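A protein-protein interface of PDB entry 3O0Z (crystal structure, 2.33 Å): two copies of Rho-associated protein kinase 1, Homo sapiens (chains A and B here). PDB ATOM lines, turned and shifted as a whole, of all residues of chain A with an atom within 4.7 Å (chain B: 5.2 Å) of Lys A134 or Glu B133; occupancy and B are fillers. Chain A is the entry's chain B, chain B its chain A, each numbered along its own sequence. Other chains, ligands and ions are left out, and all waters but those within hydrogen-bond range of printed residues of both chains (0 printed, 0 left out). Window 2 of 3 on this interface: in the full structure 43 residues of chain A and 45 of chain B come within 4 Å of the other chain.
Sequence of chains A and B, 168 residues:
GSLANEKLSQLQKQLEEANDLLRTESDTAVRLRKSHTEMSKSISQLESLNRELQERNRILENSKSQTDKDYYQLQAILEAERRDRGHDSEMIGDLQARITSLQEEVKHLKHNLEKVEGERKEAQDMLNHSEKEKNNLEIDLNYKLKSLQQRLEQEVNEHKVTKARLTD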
ATOM      1  N   SER A 130     -25.464  30.891  10.725  1.00  0.00           N
ATOM      2  CA  SER A 130     -24.932  29.571  11.024  1.00  0.00           C
ATOM      3  C   SER A 130     -25.369  28.516  10.000  1.00  0.00           C
ATOM      4  O   SER A 130     -24.535  27.796   9.445  1.00  0.00           O
ATOM      5  CB  SER A 130     -25.355  29.173  12.442  1.00  0.00           C
ATOM      6  OG  SER A 130     -24.730  27.978  12.873  1.00  0.00           O
ATOM      7  N   GLU A 131     -26.663  28.420   9.720  1.00  0.00           N
ATOM      8  CA  GLU A 131     -27.085  27.444   8.715  1.00  0.00           C
ATOM      9  C   GLU A 131     -26.523  27.773   7.341  1.00  0.00           C
ATOM     10  O   GLU A 131     -26.206  26.876   6.568  1.00  0.00           O
ATOM     11  CB  GLU A 131     -28.604  27.314   8.640  1.00  0.00           C
ATOM     12  CG  GLU A 131     -29.220  26.631   9.851  1.00  0.00           C
ATOM     13  CD  GLU A 131     -28.723  25.207  10.051  1.00  0.00           C
ATOM     14  OE1 GLU A 131     -28.431  24.534   9.036  1.00  0.00           O
ATOM     15  OE2 GLU A 131     -28.643  24.759  11.225  1.00  0.00           O
ATOM     16  N   LYS A 132     -26.413  29.060   7.037  1.00  0.00           N
ATOM     17  CA  LYS A 132     -25.895  29.476   5.746  1.00  0.00           C
ATOM     18  C   LYS A 132     -24.391  29.176   5.647  1.00  0.00           C
ATOM     19  O   LYS A 132     -23.912  28.693   4.622  1.00  0.00           O
ATOM     20  CB  LYS A 132     -26.170  30.958   5.498  1.00  0.00           C
ATOM     21  CG  LYS A 132     -25.799  31.412   4.098  1.00  0.00           C
ATOM     22  CD  LYS A 132     -25.142  32.789   4.098  1.00  0.00           C
ATOM     23  CE  LYS A 132     -26.137  33.875   4.520  1.00  0.00           C
ATOM     24  NZ  LYS A 132     -25.643  35.260   4.240  1.00  0.00           N
ATOM     25  N   GLU A 133     -23.646  29.456   6.709  1.00  0.00           N
ATOM     26  CA  GLU A 133     -22.224  29.157   6.707  1.00  0.00           C
ATOM     27  C   GLU A 133     -21.983  27.657   6.475  1.00  0.00           C
ATOM     28  O   GLU A 133     -21.210  27.263   5.584  1.00  0.00           O
ATOM     29  CB  GLU A 133     -21.572  29.622   8.015  1.00  0.00           C
ATOM     30  CG  GLU A 133     -21.272  31.123   8.076  1.00  0.00           C
ATOM     31  CD  GLU A 133     -20.436  31.606   6.886  1.00  0.00           C
ATOM     32  OE1 GLU A 133     -19.203  31.343   6.851  1.00  0.00           O
ATOM     33  OE2 GLU A 133     -21.016  32.260   5.987  1.00  0.00           O
ATOM     34  N   LYS A 134     -22.664  26.831   7.265  1.00  0.00           N
ATOM     35  CA  LYS A 134     -22.546  25.383   7.170  1.00  0.00           C
ATOM     36  C   LYS A 134     -22.902  24.866   5.786  1.00  0.00           C
ATOM     37  O   LYS A 134     -22.129  24.133   5.178  1.00  0.00           O
ATOM     38  CB  LYS A 134     -23.402  24.686   8.236  1.00  0.00           C
ATOM     39  CG  LYS A 134     -23.435  23.160   8.132  1.00  0.00           C
ATOM     40  CD  LYS A 134     -24.011  22.498   9.402  1.00  0.00           C
ATOM     41  CE  LYS A 134     -25.545  22.542   9.458  1.00  0.00           C
ATOM     42  NZ  LYS A 134     -26.041  23.237  10.697  1.00  0.00           N
ATOM     43  N   ASN A 135     -24.062  25.243   5.274  1.00  0.00           N
ATOM     44  CA  ASN A 135     -24.466  24.704   3.988  1.00  0.00           C
ATOM     45  C   ASN A 135     -23.646  25.188   2.812  1.00  0.00           C
ATOM     46  O   ASN A 135     -23.543  24.490   1.807  1.00  0.00           O
ATOM     47  CB  ASN A 135     -25.957  24.879   3.729  1.00  0.00           C
ATOM     48  CG  ASN A 135     -26.714  23.577   3.905  1.00  0.00           C
ATOM     49  OD1 ASN A 135     -26.699  22.715   3.016  1.00  0.00           O
ATOM     50  ND2 ASN A 135     -27.350  23.409   5.070  1.00  0.00           N
ATOM     51  N   ASN A 136     -23.062  26.373   2.927  1.00  0.00           N
ATOM     52  CA  ASN A 136     -22.128  26.817   1.902  1.00  0.00           C
ATOM     53  C   ASN A 136     -20.843  25.974   1.957  1.00  0.00           C
ATOM     54  O   ASN A 136     -20.344  25.539   0.945  1.00  0.00           O
ATOM     55  CB  ASN A 136     -21.817  28.309   2.039  1.00  0.00           C
ATOM     56  CG  ASN A 136     -22.972  29.184   1.604  1.00  0.00           C
ATOM     57  OD1 ASN A 136     -23.936  28.707   0.997  1.00  0.00           O
ATOM     58  ND2 ASN A 136     -22.888  30.472   1.923  1.00  0.00           N
ATOM     59  N   LEU A 137     -20.344  25.742   3.164  1.00  0.00           N
ATOM     60  CA  LEU A 137     -19.189  24.896   3.402  1.00  0.00           C
ATOM     61  C   LEU A 137     -19.410  23.498   2.855  1.00  0.00           C
ATOM     62  O   LEU A 137     -18.624  23.015   2.066  1.00  0.00           O
ATOM     63  CB  LEU A 137     -18.914  24.808   4.904  1.00  0.00           C
ATOM     64  CG  LEU A 137     -17.716  23.935   5.229  1.00  0.00           C
ATOM     65  CD1 LEU A 137     -16.592  24.335   4.314  1.00  0.00           C
ATOM     66  CD2 LEU A 137     -17.324  24.081   6.678  1.00  0.00           C
ATOM     67  N   GLU A 138     -20.484  22.846   3.281  1.00  0.00           N
ATOM     68  CA  GLU A 138     -20.816  21.513   2.782  1.00  0.00           C
ATOM     69  C   GLU A 138     -20.945  21.495   1.256  1.00  0.00           C
ATOM     70  O   GLU A 138     -20.537  20.549   0.601  1.00  0.00           O
ATOM     71  CB  GLU A 138     -22.126  21.016   3.401  1.00  0.00           C
ATOM     72  CG  GLU A 138     -22.049  20.670   4.880  1.00  0.00           C
ATOM     73  CD  GLU A 138     -23.404  20.311   5.480  1.00  0.00           C
ATOM     74  OE1 GLU A 138     -24.440  20.565   4.820  1.00  0.00           O
ATOM     75  OE2 GLU A 138     -23.433  19.788   6.621  1.00  0.00           O
ATOM     76  N   ASN B 128     -28.543  26.829  19.161  1.00  0.00           N
ATOM     77  CA  ASN B 128     -27.543  26.002  19.823  1.00  0.00           C
ATOM     78  C   ASN B 128     -27.281  24.740  19.035  1.00  0.00           C
ATOM     79  O   ASN B 128     -26.133  24.353  18.816  1.00  0.00           O
ATOM     80  CB  ASN B 128     -27.962  25.634  21.239  1.00  0.00           C
ATOM     81  CG  ASN B 128     -27.801  26.783  22.210  1.00  0.00           C
ATOM     82  OD1 ASN B 128     -26.999  27.697  21.981  1.00  0.00           O
ATOM     83  ND2 ASN B 128     -28.563  26.743  23.314  1.00  0.00           N
ATOM     84  N   HIS B 129     -28.360  24.098  18.612  1.00  0.00           N
ATOM     85  CA  HIS B 129     -28.242  22.878  17.847  1.00  0.00           C
ATOM     86  C   HIS B 129     -27.490  23.155  16.556  1.00  0.00           C
ATOM     87  O   HIS B 129     -26.655  22.378  16.155  1.00  0.00           O
ATOM     88  CB  HIS B 129     -29.622  22.336  17.547  1.00  0.00           C
ATOM     89  CG  HIS B 129     -29.621  21.156  16.633  1.00  0.00           C
ATOM     90  ND1 HIS B 129     -30.286  21.152  15.427  1.00  0.00           N
ATOM     91  CD2 HIS B 129     -29.052  19.933  16.758  1.00  0.00           C
ATOM     92  CE1 HIS B 129     -30.134  19.971  14.849  1.00  0.00           C
ATOM     93  NE2 HIS B 129     -29.391  19.216  15.635  1.00  0.00           N
ATOM     94  N   SER B 130     -27.776  24.280  15.912  1.00  0.00           N
ATOM     95  CA  SER B 130     -27.104  24.605  14.669  1.00  0.00           C
ATOM     96  C   SER B 130     -25.611  24.810  14.922  1.00  0.00           C
ATOM     97  O   SER B 130     -24.774  24.360  14.146  1.00  0.00           O
ATOM     98  CB  SER B 130     -27.697  25.861  14.029  1.00  0.00           C
ATOM     99  OG  SER B 130     -26.972  26.245  12.860  1.00  0.00           O
ATOM    100  N   GLU B 131     -25.275  25.490  16.010  1.00  0.00           N
ATOM    101  CA  GLU B 131     -23.877  25.745  16.298  1.00  0.00           C
ATOM    102  C   GLU B 131     -23.121  24.461  16.633  1.00  0.00           C
ATOM    103  O   GLU B 131     -22.007  24.265  16.161  1.00  0.00           O
ATOM    104  CB  GLU B 131     -23.707  26.817  17.381  1.00  0.00           C
ATOM    105  CG  GLU B 131     -23.812  28.247  16.815  1.00  0.00           C
ATOM    106  CD  GLU B 131     -23.755  29.343  17.882  1.00  0.00           C
ATOM    107  OE1 GLU B 131     -23.843  29.009  19.090  1.00  0.00           O
ATOM    108  OE2 GLU B 131     -23.629  30.539  17.503  1.00  0.00           O
ATOM    109  N   LYS B 132     -23.723  23.586  17.431  1.00  0.00           N
ATOM    110  CA  LYS B 132     -23.070  22.330  17.762  1.00  0.00           C
ATOM    111  C   LYS B 132     -22.889  21.473  16.498  1.00  0.00           C
ATOM    112  O   LYS B 132     -21.797  20.976  16.205  1.00  0.00           O
ATOM    113  CB  LYS B 132     -23.835  21.566  18.850  1.00  0.00           C
ATOM    114  CG  LYS B 132     -23.757  22.210  20.225  1.00  0.00           C
ATOM    115  CD  LYS B 132     -24.148  21.236  21.313  1.00  0.00           C
ATOM    116  CE  LYS B 132     -24.238  21.904  22.675  1.00  0.00           C
ATOM    117  NZ  LYS B 132     -25.613  22.489  22.900  1.00  0.00           N
ATOM    118  N   GLU B 133     -23.959  21.310  15.737  1.00  0.00           N
ATOM    119  CA  GLU B 133     -23.900  20.528  14.512  1.00  0.00           C
ATOM    120  C   GLU B 133     -22.804  21.046  13.572  1.00  0.00           C
ATOM    121  O   GLU B 133     -22.046  20.265  12.975  1.00  0.00           O
ATOM    122  CB  GLU B 133     -25.289  20.535  13.873  1.00  0.00           C
ATOM    123  CG  GLU B 133     -25.387  20.148  12.427  1.00  0.00           C
ATOM    124  CD  GLU B 133     -26.830  19.874  12.029  1.00  0.00           C
ATOM    125  OE1 GLU B 133     -27.144  19.957  10.813  1.00  0.00           O
ATOM    126  OE2 GLU B 133     -27.642  19.583  12.943  1.00  0.00           O
ATOM    127  N   LYS B 134     -22.697  22.363  13.468  1.00  0.00           N
ATOM    128  CA  LYS B 134     -21.681  22.984  12.628  1.00  0.00           C
ATOM    129  C   LYS B 134     -20.291  22.769  13.208  1.00  0.00           C
ATOM    130  O   LYS B 134     -19.302  22.639  12.488  1.00  0.00           O
ATOM    131  CB  LYS B 134     -21.937  24.488  12.491  1.00  0.00           C
ATOM    132  CG  LYS B 134     -21.062  25.159  11.440  1.00  0.00           C
ATOM    133  CD  LYS B 134     -21.563  26.548  11.096  1.00  0.00           C
ATOM    134  CE  LYS B 134     -21.167  27.537  12.158  1.00  0.00           C
ATOM    135  NZ  LYS B 134     -19.697  27.588  12.175  1.00  0.00           N
ATOM    136  N   ASN B 135     -20.221  22.755  14.526  1.00  0.00           N
ATOM    137  CA  ASN B 135     -18.954  22.577  15.204  1.00  0.00           C
ATOM    138  C   ASN B 135     -18.421  21.161  14.994  1.00  0.00           C
ATOM    139  O   ASN B 135     -17.231  20.935  14.850  1.00  0.00           O
ATOM    140  CB  ASN B 135     -19.181  22.804  16.684  1.00  0.00           C
ATOM    141  CG  ASN B 135     -17.909  22.968  17.432  1.00  0.00           C
ATOM    142  OD1 ASN B 135     -17.062  23.783  17.048  1.00  0.00           O
ATOM    143  ND2 ASN B 135     -17.754  22.210  18.518  1.00  0.00           N
ATOM    144  N   ASN B 136     -19.334  20.207  15.021  1.00  0.00           N
ATOM    145  CA  ASN B 136     -19.004  18.828  14.840  1.00  0.00           C
ATOM    146  C   ASN B 136     -18.501  18.662  13.422  1.00  0.00           C
ATOM    147  O   ASN B 136     -17.527  17.964  13.183  1.00  0.00           O
ATOM    148  CB  ASN B 136     -20.235  17.954  15.076  1.00  0.00           C
ATOM    149  CG  ASN B 136     -20.596  17.836  16.546  1.00  0.00           C
ATOM    150  OD1 ASN B 136     -19.792  18.137  17.427  1.00  0.00           O
ATOM    151  ND2 ASN B 136     -21.801  17.370  16.814  1.00  0.00           N
ATOM    152  N   LEU B 137     -19.160  19.330  12.489  1.00  0.00           N
ATOM    153  CA  LEU B 137     -18.761  19.270  11.091  1.00  0.00           C
ATOM    154  C   LEU B 137     -17.324  19.759  10.949  1.00  0.00           C
ATOM    155  O   LEU B 137     -16.463  19.053  10.436  1.00  0.00           O
ATOM    156  CB  LEU B 137     -19.697  20.124  10.232  1.00  0.00           C
ATOM    157  CG  LEU B 137     -19.395  20.151   8.747  1.00  0.00           C
ATOM    158  CD1 LEU B 137     -19.193  18.743   8.312  1.00  0.00           C
ATOM    159  CD2 LEU B 137     -20.554  20.739   8.016  1.00  0.00           C
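Ser B130 touches its own counterpart, Ser A130. Glu A131 touches Ser B130, but with the chains exchanged Ser A130 does not touch Glu B131 (4.04 Å). Lys A134 touches Glu B133, but with the chains exchanged Glu A133 does not touch Lys B134 (4.4 Å). Lys A134 touches its own counterpart, Lys B134. 8 positions are printed for both chains. Of the 8 pairs that touch across the chains among the printed residues, 4 have their exchanged pair printed and touching as well.
The side-chain carboxylate (OE2) of Glu B133 sits close to a ring nitrogen (NE2) of His B129. The side-chain amino group (NZ) of Lys A134 lies within salt-bridge range of the side-chain carboxylate (OE2) of Glu A131 (3.1 Å).
Hydrophobic or aromatic side chains of chain B that line the printed part of chain A: Leu B137. Along chain B the printed residues that touch a printed residue of chain A span positions 130 to 137. Along chain A the printed residues that touch a printed residue of chain B span positions 130 to 138. Among the printed residues, 8 pairs touch across the chains. Among the printed residues, Asp or Glu carboxylates within 4 Å of a Lys or Arg side-chain nitrogen of the other chain: Lys A134 with Glu B133.
Among the printed residues, pairs that only touch across the chains: Ser A130 with Lys B134, Lys A134 with Ser B130, Lys A134 with Lys B134, Lys A134 with Leu B137 and Glu A138 with Leu B137.
Printed residues of chain B within 4 Å of Ser A130: Ser B130 (2.8 Å) and Lys B134 (3.6 Å). Lys A134 touches just these residues of chain B: Ser B130, Glu B133, Lys B134 and Leu B137. Of the printed residues of chain B, Glu A138 touches Leu B137. Glu B133 touches one residue of chain A. The nearest printed residue of chain B that does not touch Lys A134 is His B129 (5.6 Å).
OG of Ser B130 lies within hydrogen-bond range of OG of Ser A130, at 2.8 Å. OG of Ser B130 sits at hydrogen-bond distance from OE2 of Glu A131. The side-chain amino group (NZ) of Lys A134 is in salt-bridge range of the side-chain carboxylate (OE1) of Glu B133 (3.5 Å).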
